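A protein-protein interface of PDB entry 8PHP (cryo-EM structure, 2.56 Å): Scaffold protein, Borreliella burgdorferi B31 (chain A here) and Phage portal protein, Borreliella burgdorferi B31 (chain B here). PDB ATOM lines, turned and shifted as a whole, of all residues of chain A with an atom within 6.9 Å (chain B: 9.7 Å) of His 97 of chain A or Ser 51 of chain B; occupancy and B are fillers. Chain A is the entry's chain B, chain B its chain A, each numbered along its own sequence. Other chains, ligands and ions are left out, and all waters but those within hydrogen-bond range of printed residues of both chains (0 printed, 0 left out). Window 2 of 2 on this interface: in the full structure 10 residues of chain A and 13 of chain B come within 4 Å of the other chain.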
ATOM      1  N   LEU A  94     -11.430   2.475  26.452  1.00  0.00           N
ATOM      2  CA  LEU A  94     -10.601   2.778  25.298  1.00  0.00           C
ATOM      3  C   LEU A  94     -10.861   1.779  24.172  1.00  0.00           C
ATOM      4  O   LEU A  94     -11.473   0.726  24.365  1.00  0.00           O
ATOM      5  CB  LEU A  94      -9.119   2.773  25.680  1.00  0.00           C
ATOM      6  CG  LEU A  94      -8.700   3.773  26.765  1.00  0.00           C
ATOM      7  CD1 LEU A  94      -7.203   3.700  27.030  1.00  0.00           C
ATOM      8  CD2 LEU A  94      -9.112   5.191  26.389  1.00  0.00           C
ATOM      9  N   SER A  95     -10.391   2.133  22.981  1.00  0.00           N
ATOM     10  CA  SER A  95     -10.559   1.289  21.809  1.00  0.00           C
ATOM     11  C   SER A  95      -9.708   0.026  21.923  1.00  0.00           C
ATOM     12  O   SER A  95      -8.746  -0.046  22.691  1.00  0.00           O
ATOM     13  CB  SER A  95     -10.182   2.054  20.539  1.00  0.00           C
ATOM     14  OG  SER A  95     -10.160   1.195  19.413  1.00  0.00           O
ATOM     15  N   ASN A  96     -10.081  -0.982  21.131  1.00  0.00           N
ATOM     16  CA  ASN A  96      -9.293  -2.206  21.054  1.00  0.00           C
ATOM     17  C   ASN A  96      -7.934  -1.983  20.403  1.00  0.00           C
ATOM     18  O   ASN A  96      -7.089  -2.884  20.445  1.00  0.00           O
ATOM     19  CB  ASN A  96     -10.066  -3.284  20.288  1.00  0.00           C
ATOM     20  CG  ASN A  96     -10.551  -2.803  18.937  1.00  0.00           C
ATOM     21  OD1 ASN A  96     -10.340  -1.650  18.562  1.00  0.00           O
ATOM     22  ND2 ASN A  96     -11.209  -3.687  18.197  1.00  0.00           N
ATOM     23  N   HIS A  97      -7.710  -0.816  19.794  1.00  0.00           N
ATOM     24  CA  HIS A  97      -6.390  -0.480  19.276  1.00  0.00           C
ATOM     25  C   HIS A  97      -5.381  -0.262  20.396  1.00  0.00           C
ATOM     26  O   HIS A  97      -4.173  -0.382  20.162  1.00  0.00           O
ATOM     27  CB  HIS A  97      -6.492   0.763  18.385  1.00  0.00           C
ATOM     28  CG  HIS A  97      -5.182   1.437  18.121  1.00  0.00           C
ATOM     29  ND1 HIS A  97      -4.238   0.919  17.261  1.00  0.00           N
ATOM     30  CD2 HIS A  97      -4.664   2.594  18.597  1.00  0.00           C
ATOM     31  CE1 HIS A  97      -3.191   1.725  17.223  1.00  0.00           C
ATOM     32  NE2 HIS A  97      -3.425   2.749  18.024  1.00  0.00           N
ATOM     33  N   PHE A  98      -5.850   0.024  21.611  1.00  0.00           N
ATOM     34  CA  PHE A  98      -4.993   0.204  22.776  1.00  0.00           C
ATOM     35  C   PHE A  98      -4.907  -1.059  23.628  1.00  0.00           C
ATOM     36  O   PHE A  98      -4.639  -0.981  24.832  1.00  0.00           O
ATOM     37  CB  PHE A  98      -5.486   1.379  23.621  1.00  0.00           C
ATOM     38  CG  PHE A  98      -5.495   2.690  22.892  1.00  0.00           C
ATOM     39  CD1 PHE A  98      -4.320   3.399  22.704  1.00  0.00           C
ATOM     40  CD2 PHE A  98      -6.676   3.219  22.400  1.00  0.00           C
ATOM     41  CE1 PHE A  98      -4.323   4.608  22.034  1.00  0.00           C
ATOM     42  CE2 PHE A  98      -6.687   4.426  21.730  1.00  0.00           C
ATOM     43  CZ  PHE A  98      -5.509   5.123  21.547  1.00  0.00           C
ATOM     44  N   ASN A  99      -5.137  -2.221  23.026  1.00  0.00           N
ATOM     45  CA  ASN A  99      -5.074  -3.482  23.748  1.00  0.00           C
ATOM     46  C   ASN A  99      -3.621  -3.867  24.000  1.00  0.00           C
ATOM     47  O   ASN A  99      -2.747  -3.625  23.164  1.00  0.00           O
ATOM     48  CB  ASN A  99      -5.786  -4.582  22.960  1.00  0.00           C
ATOM     49  CG  ASN A  99      -5.767  -5.919  23.676  1.00  0.00           C
ATOM     50  OD1 ASN A  99      -5.593  -6.969  23.055  1.00  0.00           O
ATOM     51  ND2 ASN A  99      -5.964  -5.889  24.990  1.00  0.00           N
ATOM     52  N   LYS A 100      -3.369  -4.463  25.168  1.00  0.00           N
ATOM     53  CA  LYS A 100      -2.006  -4.820  25.550  1.00  0.00           C
ATOM     54  C   LYS A 100      -1.334  -5.712  24.514  1.00  0.00           C
ATOM     55  O   LYS A 100      -0.125  -5.597  24.285  1.00  0.00           O
ATOM     56  CB  LYS A 100      -2.013  -5.510  26.915  1.00  0.00           C
ATOM     57  CG  LYS A 100      -2.451  -4.610  28.060  1.00  0.00           C
ATOM     58  CD  LYS A 100      -2.425  -5.352  29.385  1.00  0.00           C
ATOM     59  CE  LYS A 100      -1.986  -4.441  30.519  1.00  0.00           C
ATOM     60  NZ  LYS A 100      -0.657  -3.823  30.264  1.00  0.00           N
ATOM     61  N   VAL A 102      -1.860  -5.896  21.084  1.00  0.00           N
ATOM     62  CA  VAL A 102      -1.453  -5.170  19.885  1.00  0.00           C
ATOM     63  C   VAL A 102      -0.407  -4.111  20.215  1.00  0.00           C
ATOM     64  O   VAL A 102       0.470  -3.819  19.392  1.00  0.00           O
ATOM     65  CB  VAL A 102      -2.677  -4.560  19.173  1.00  0.00           C
ATOM     66  CG1 VAL A 102      -3.543  -5.660  18.578  1.00  0.00           C
ATOM     67  CG2 VAL A 102      -3.486  -3.699  20.125  1.00  0.00           C
ATOM     68  N   LEU A 103      -0.481  -3.512  21.406  1.00  0.00           N
ATOM     69  CA  LEU A 103       0.542  -2.551  21.811  1.00  0.00           C
ATOM     70  C   LEU A 103       1.902  -3.222  21.955  1.00  0.00           C
ATOM     71  O   LEU A 103       2.932  -2.635  21.603  1.00  0.00           O
ATOM     72  CB  LEU A 103       0.138  -1.863  23.115  1.00  0.00           C
ATOM     73  CG  LEU A 103      -1.078  -0.935  23.064  1.00  0.00           C
ATOM     74  CD1 LEU A 103      -1.168  -0.094  24.327  1.00  0.00           C
ATOM     75  CD2 LEU A 103      -1.028  -0.048  21.832  1.00  0.00           C
ATOM     76  N   LYS A 106       3.617  -3.584  18.556  1.00  0.00           N
ATOM     77  CA  LYS A 106       4.244  -2.370  18.050  1.00  0.00           C
ATOM     78  C   LYS A 106       5.580  -2.067  18.717  1.00  0.00           C
ATOM     79  O   LYS A 106       6.316  -1.209  18.220  1.00  0.00           O
ATOM     80  CB  LYS A 106       3.298  -1.180  18.222  1.00  0.00           C
ATOM     81  CG  LYS A 106       2.215  -1.092  17.158  1.00  0.00           C
ATOM     82  CD  LYS A 106       1.389   0.176  17.309  1.00  0.00           C
ATOM     83  CE  LYS A 106       0.365   0.038  18.422  1.00  0.00           C
ATOM     84  NZ  LYS A 106      -0.623  -1.039  18.138  1.00  0.00           N
ATOM     85  N   LEU B  43      -7.231   9.929   5.485  1.00  0.00           N
ATOM     86  CA  LEU B  43      -7.447  10.028   6.921  1.00  0.00           C
ATOM     87  C   LEU B  43      -6.100  10.052   7.628  1.00  0.00           C
ATOM     88  O   LEU B  43      -5.234   9.216   7.350  1.00  0.00           O
ATOM     89  CB  LEU B  43      -8.300   8.864   7.432  1.00  0.00           C
ATOM     90  CG  LEU B  43      -9.089   9.122   8.717  1.00  0.00           C
ATOM     91  CD1 LEU B  43      -9.890  10.408   8.606  1.00  0.00           C
ATOM     92  CD2 LEU B  43     -10.001   7.948   9.029  1.00  0.00           C
ATOM     93  N   GLU B  44      -5.927  11.010   8.536  1.00  0.00           N
ATOM     94  CA  GLU B  44      -4.677  11.178   9.260  1.00  0.00           C
ATOM     95  C   GLU B  44      -4.970  11.437  10.729  1.00  0.00           C
ATOM     96  O   GLU B  44      -6.034  11.950  11.085  1.00  0.00           O
ATOM     97  CB  GLU B  44      -3.841  12.327   8.683  1.00  0.00           C
ATOM     98  CG  GLU B  44      -3.030  11.951   7.456  1.00  0.00           C
ATOM     99  CD  GLU B  44      -2.423  13.157   6.769  1.00  0.00           C
ATOM    100  OE1 GLU B  44      -2.984  14.264   6.904  1.00  0.00           O
ATOM    101  OE2 GLU B  44      -1.385  12.998   6.094  1.00  0.00           O
ATOM    102  N   SER B  45      -4.012  11.079  11.579  1.00  0.00           N
ATOM    103  CA  SER B  45      -4.113  11.276  13.018  1.00  0.00           C
ATOM    104  C   SER B  45      -3.081  12.302  13.461  1.00  0.00           C
ATOM    105  O   SER B  45      -1.894  12.173  13.141  1.00  0.00           O
ATOM    106  CB  SER B  45      -3.907   9.958  13.768  1.00  0.00           C
ATOM    107  OG  SER B  45      -2.617   9.429  13.522  1.00  0.00           O
ATOM    108  N   ALA B  47      -2.064  12.893  16.552  1.00  0.00           N
ATOM    109  CA  ALA B  47      -1.164  12.288  17.527  1.00  0.00           C
ATOM    110  C   ALA B  47      -0.135  11.370  16.881  1.00  0.00           C
ATOM    111  O   ALA B  47       0.899  11.092  17.499  1.00  0.00           O
ATOM    112  CB  ALA B  47      -1.965  11.513  18.574  1.00  0.00           C
ATOM    113  N   HIS B  48      -0.395  10.900  15.659  1.00  0.00           N
ATOM    114  CA  HIS B  48       0.509  10.000  14.939  1.00  0.00           C
ATOM    115  C   HIS B  48       0.798   8.738  15.751  1.00  0.00           C
ATOM    116  O   HIS B  48       1.922   8.232  15.775  1.00  0.00           O
ATOM    117  CB  HIS B  48       1.809  10.713  14.555  1.00  0.00           C
ATOM    118  CG  HIS B  48       2.571  10.032  13.460  1.00  0.00           C
ATOM    119  ND1 HIS B  48       2.039   9.816  12.207  1.00  0.00           N
ATOM    120  CD2 HIS B  48       3.823   9.519  13.432  1.00  0.00           C
ATOM    121  CE1 HIS B  48       2.931   9.199  11.454  1.00  0.00           C
ATOM    122  NE2 HIS B  48       4.023   9.007  12.172  1.00  0.00           N
ATOM    123  N   ASN B  49      -0.232   8.226  16.426  1.00  0.00           N
ATOM    124  CA  ASN B  49      -0.114   7.014  17.222  1.00  0.00           C
ATOM    125  C   ASN B  49      -0.980   5.866  16.730  1.00  0.00           C
ATOM    126  O   ASN B  49      -0.689   4.713  17.067  1.00  0.00           O
ATOM    127  CB  ASN B  49      -0.464   7.299  18.692  1.00  0.00           C
ATOM    128  CG  ASN B  49       0.635   8.047  19.419  1.00  0.00           C
ATOM    129  OD1 ASN B  49       1.701   8.303  18.859  1.00  0.00           O
ATOM    130  ND2 ASN B  49       0.382   8.401  20.672  1.00  0.00           N
ATOM    131  N   VAL B  50      -2.023   6.139  15.954  1.00  0.00           N
ATOM    132  CA  VAL B  50      -2.898   5.091  15.443  1.00  0.00           C
ATOM    133  C   VAL B  50      -2.201   4.365  14.301  1.00  0.00           C
ATOM    134  O   VAL B  50      -1.596   4.988  13.422  1.00  0.00           O
ATOM    135  CB  VAL B  50      -4.243   5.685  14.989  1.00  0.00           C
ATOM    136  CG1 VAL B  50      -5.249   4.575  14.720  1.00  0.00           C
ATOM    137  CG2 VAL B  50      -4.772   6.653  16.034  1.00  0.00           C
ATOM    138  N   SER B  51      -2.281   3.037  14.316  1.00  0.00           N
ATOM    139  CA  SER B  51      -1.702   2.239  13.247  1.00  0.00           C
ATOM    140  C   SER B  51      -2.449   2.475  11.939  1.00  0.00           C
ATOM    141  O   SER B  51      -3.647   2.769  11.924  1.00  0.00           O
ATOM    142  CB  SER B  51      -1.735   0.755  13.609  1.00  0.00           C
ATOM    143  OG  SER B  51      -3.067   0.295  13.758  1.00  0.00           O
ATOM    144  N   GLU B  52      -1.721   2.344  10.828  1.00  0.00           N
ATOM    145  CA  GLU B  52      -2.324   2.573   9.519  1.00  0.00           C
ATOM    146  C   GLU B  52      -3.381   1.527   9.190  1.00  0.00           C
ATOM    147  O   GLU B  52      -4.363   1.839   8.508  1.00  0.00           O
ATOM    148  CB  GLU B  52      -1.245   2.593   8.437  1.00  0.00           C
ATOM    149  CG  GLU B  52      -0.259   3.739   8.568  1.00  0.00           C
ATOM    150  CD  GLU B  52       0.793   3.730   7.478  1.00  0.00           C
ATOM    151  OE1 GLU B  52       0.779   2.799   6.644  1.00  0.00           O
ATOM    152  OE2 GLU B  52       1.634   4.652   7.453  1.00  0.00           O
ATOM    153  N   VAL B  53      -3.196   0.289   9.651  1.00  0.00           N
ATOM    154  CA  VAL B  53      -4.180  -0.758   9.386  1.00  0.00           C
ATOM    155  C   VAL B  53      -5.509  -0.415  10.046  1.00  0.00           C
ATOM    156  O   VAL B  53      -6.577  -0.530   9.432  1.00  0.00           O
ATOM    157  CB  VAL B  53      -3.651  -2.123   9.860  1.00  0.00           C
ATOM    158  CG1 VAL B  53      -4.687  -3.209   9.609  1.00  0.00           C
ATOM    159  CG2 VAL B  53      -2.342  -2.455   9.164  1.00  0.00           C
ATOM    160  N   GLU B  54      -5.463   0.012  11.309  1.00  0.00           N
ATOM    161  CA  GLU B  54      -6.680   0.428  11.998  1.00  0.00           C
ATOM    162  C   GLU B  54      -7.252   1.698  11.380  1.00  0.00           C
ATOM    163  O   GLU B  54      -8.466   1.810  11.177  1.00  0.00           O
ATOM    164  CB  GLU B  54      -6.395   0.633  13.487  1.00  0.00           C
ATOM    165  CG  GLU B  54      -7.467   1.414  14.235  1.00  0.00           C
ATOM    166  CD  GLU B  54      -8.733   0.610  14.480  1.00  0.00           C
ATOM    167  OE1 GLU B  54      -8.775  -0.580  14.103  1.00  0.00           O
ATOM    168  OE2 GLU B  54      -9.690   1.171  15.054  1.00  0.00           O
ATOM    169  N   LEU B  55      -6.386   2.666  11.074  1.00  0.00           N
ATOM    170  CA  LEU B  55      -6.850   3.933  10.517  1.00  0.00           C
ATOM    171  C   LEU B  55      -7.496   3.743   9.151  1.00  0.00           C
ATOM    172  O   LEU B  55      -8.453   4.451   8.814  1.00  0.00           O
ATOM    173  CB  LEU B  55      -5.685   4.918  10.425  1.00  0.00           C
ATOM    174  CG  LEU B  55      -6.015   6.350  10.010  1.00  0.00           C
ATOM    175  CD1 LEU B  55      -6.952   6.992  11.018  1.00  0.00           C
ATOM    176  CD2 LEU B  55      -4.741   7.164   9.867  1.00  0.00           C
ATOM    177  N   ALA B  56      -6.992   2.801   8.352  1.00  0.00           N
ATOM    178  CA  ALA B  56      -7.595   2.536   7.050  1.00  0.00           C
ATOM    179  C   ALA B  56      -9.000   1.966   7.196  1.00  0.00           C
ATOM    180  O   ALA B  56      -9.894   2.297   6.409  1.00  0.00           O
ATOM    181  CB  ALA B  56      -6.711   1.584   6.243  1.00  0.00           C
ATOM    182  N   ARG B  57      -9.212   1.101   8.191  1.00  0.00           N
ATOM    183  CA  ARG B  57     -10.541   0.540   8.416  1.00  0.00           C
ATOM    184  C   ARG B  57     -11.535   1.623   8.817  1.00  0.00           C
ATOM    185  O   ARG B  57     -12.711   1.566   8.440  1.00  0.00           O
ATOM    186  CB  ARG B  57     -10.473  -0.555   9.479  1.00  0.00           C
ATOM    187  CG  ARG B  57     -11.757  -1.349   9.641  1.00  0.00           C
ATOM    188  CD  ARG B  57     -11.736  -2.180  10.915  1.00  0.00           C
ATOM    189  NE  ARG B  57     -11.560  -1.364  12.111  1.00  0.00           N
ATOM    190  CZ  ARG B  57     -12.502  -0.597  12.643  1.00  0.00           C
ATOM    191  NH1 ARG B  57     -13.713  -0.522  12.117  1.00  0.00           N
ATOM    192  NH2 ARG B  57     -12.223   0.108  13.736  1.00  0.00           N
ATOM    193  N   LEU B  58     -11.081   2.615   9.587  1.00  0.00           N
ATOM    194  CA  LEU B  58     -11.943   3.744   9.921  1.00  0.00           C
ATOM    195  C   LEU B  58     -12.332   4.524   8.673  1.00  0.00           C
ATOM    196  O   LEU B  58     -13.469   4.995   8.553  1.00  0.00           O
ATOM    197  CB  LEU B  58     -11.245   4.658  10.928  1.00  0.00           C
ATOM    198  CG  LEU B  58     -11.088   4.129  12.354  1.00  0.00           C
ATOM    199  CD1 LEU B  58     -10.733   5.257  13.306  1.00  0.00           C
ATOM    200  CD2 LEU B  58     -12.356   3.426  12.804  1.00  0.00           C
ATOM    201  N   LYS B  59     -11.394   4.678   7.734  1.00  0.00           N
ATOM    202  CA  LYS B  59     -11.686   5.401   6.502  1.00  0.00           C
ATOM    203  C   LYS B  59     -12.750   4.686   5.678  1.00  0.00           C
ATOM    204  O   LYS B  59     -13.566   5.332   5.009  1.00  0.00           O
ATOM    205  CB  LYS B  59     -10.407   5.580   5.687  1.00  0.00           C
ATOM    206  CG  LYS B  59     -10.524   6.582   4.553  1.00  0.00           C
ATOM    207  CD  LYS B  59      -9.179   6.822   3.891  1.00  0.00           C
ATOM    208  CE  LYS B  59      -8.604   5.536   3.326  1.00  0.00           C
ATOM    209  NZ  LYS B  59      -7.320   5.771   2.612  1.00  0.00           N
ATOM    210  N   LYS B  86     -16.224   3.972  22.215  1.00  0.00           N
ATOM    211  CA  LYS B  86     -16.328   2.863  23.162  1.00  0.00           C
ATOM    212  C   LYS B  86     -17.075   3.357  24.397  1.00  0.00           C
ATOM    213  O   LYS B  86     -16.496   3.676  25.438  1.00  0.00           O
ATOM    214  CB  LYS B  86     -14.948   2.321  23.511  1.00  0.00           C
ATOM    215  CG  LYS B  86     -14.964   1.061  24.364  1.00  0.00           C
ATOM    216  CD  LYS B  86     -15.607  -0.100  23.628  1.00  0.00           C
ATOM    217  CE  LYS B  86     -15.583  -1.364  24.470  1.00  0.00           C
ATOM    218  NZ  LYS B  86     -16.230  -2.508  23.773  1.00  0.00           N
ATOM    219  N   LEU B 100     -10.293   8.515  20.600  1.00  0.00           N
ATOM    220  CA  LEU B 100     -10.249   7.911  19.278  1.00  0.00           C
ATOM    221  C   LEU B 100     -11.554   7.162  19.016  1.00  0.00           C
ATOM    222  O   LEU B 100     -12.006   6.384  19.862  1.00  0.00           O
ATOM    223  CB  LEU B 100      -9.061   6.956  19.164  1.00  0.00           C
ATOM    224  CG  LEU B 100      -8.890   6.172  17.860  1.00  0.00           C
ATOM    225  CD1 LEU B 100      -8.399   7.078  16.741  1.00  0.00           C
ATOM    226  CD2 LEU B 100      -7.945   5.001  18.055  1.00  0.00           C
ATOM    227  N   PRO B 101     -12.181   7.371  17.863  1.00  0.00           N
ATOM    228  CA  PRO B 101     -13.477   6.741  17.602  1.00  0.00           C
ATOM    229  C   PRO B 101     -13.341   5.281  17.195  1.00  0.00           C
ATOM    230  O   PRO B 101     -12.278   4.807  16.796  1.00  0.00           O
ATOM    231  CB  PRO B 101     -14.042   7.579  16.453  1.00  0.00           C
ATOM    232  CG  PRO B 101     -12.833   8.023  15.713  1.00  0.00           C
ATOM    233  CD  PRO B 101     -11.763   8.247  16.756  1.00  0.00           C
ATOM    234  N   ILE B 102     -14.462   4.571  17.306  1.00  0.00           N
ATOM    235  CA  ILE B 102     -14.517   3.176  16.887  1.00  0.00           C
ATOM    236  C   ILE B 102     -15.018   3.038  15.452  1.00  0.00           C
ATOM    237  O   ILE B 102     -14.623   2.105  14.747  1.00  0.00           O
ATOM    238  CB  ILE B 102     -15.399   2.364  17.853  1.00  0.00           C
ATOM    239  CG1 ILE B 102     -15.034   2.679  19.303  1.00  0.00           C
ATOM    240  CG2 ILE B 102     -15.264   0.873  17.583  1.00  0.00           C
ATOM    241  CD1 ILE B 102     -13.614   2.335  19.658  1.00  0.00           C
ATOM    242  N   LEU B 354      -8.597  13.812  14.772  1.00  0.00           N
ATOM    243  CA  LEU B 354      -8.478  13.213  13.453  1.00  0.00           C
ATOM    244  C   LEU B 354      -8.683  14.278  12.388  1.00  0.00           C
ATOM    245  O   LEU B 354      -9.405  15.257  12.595  1.00  0.00           O
ATOM    246  CB  LEU B 354      -9.493  12.079  13.254  1.00  0.00           C
ATOM    247  CG  LEU B 354      -9.140  10.726  13.874  1.00  0.00           C
ATOM    248  CD1 LEU B 354     -10.065   9.641  13.348  1.00  0.00           C
ATOM    249  CD2 LEU B 354      -7.688  10.372  13.602  1.00  0.00           C
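Of chain B, only Ile 102 (3.6 Å) comes within 4 Å of Ser 95 of chain A. No residue of chain B comes within 4 Å of Asn 96 of chain A. Of chain B, only Asn 49, Val 50 and Ser 51 come within 4 Å of His 97 of chain A. Phe 98 of chain A touches just one residue of chain B: Leu 100. Of the printed residues of chain A, Asn 49 of chain B touches His 97. Printed residues of chain A within 4 Å of Val 50 of chain B: His 97. Ser 51 of chain B touches just one residue of chain A: His 97 (3.3 Å). Of the printed residues of chain A, Lys 86 of chain B touches Leu 94 (3.5 Å). Printed residues of chain A within 4 Å of Leu 100 of chain B: Phe 98 (3.9 Å). Of the printed residues of chain A, Ile 102 of chain B touches Ser 95 (3.6 Å). Leu 354 of chain B touches none of the printed residues of chain A.
Hydrophobic or aromatic side chains of chain A within 4 Å of the printed part of chain B: His 97 and Phe 98. Of the 21 printed residues of chain B, 6 touch a printed residue of chain A. Hydrophobic or aromatic side chains of chain B within 4 Å of the printed part of chain A: Leu 100 and Ile 102.
O of Ala 47 of chain B sits close to OD1 of Asn 49 of chain B, at 3.2 Å. OG of Ser 51 of chain B lies close to N of Glu 54 of chain B, 3.4 Å away. The backbone carbonyl oxygen (O) of Ile 102 of chain B lies within hydrogen-bond range of the guanidinium group (NH2) of Arg 57 of chain B (3.3 Å). OG of Ser 95 of chain A lies within hydrogen-bond range of OD1 of Asn 96 of chain A, 3.0 Å away. N of His 97 of chain A lies close to OG of Ser 95 of chain A (3.2 Å).
O of Leu 94 of chain A touches CG of Lys 86 of chain B, 3.5 Å away. CB of Ser 95 of chain A touches CD1 of Ile 102 of chain B (3.6 Å). His 97 of chain A touches Asn 49 of chain B (NE2 to O, 3.5 Å). Val 50 of chain B touches His 97 of chain A. CE1 of His 97 of chain A touches N of Ser 51 of chain B, 3.3 Å away. CE2 of Phe 98 of chain A touches CD2 of Leu 100 of chain B (3.9 Å).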
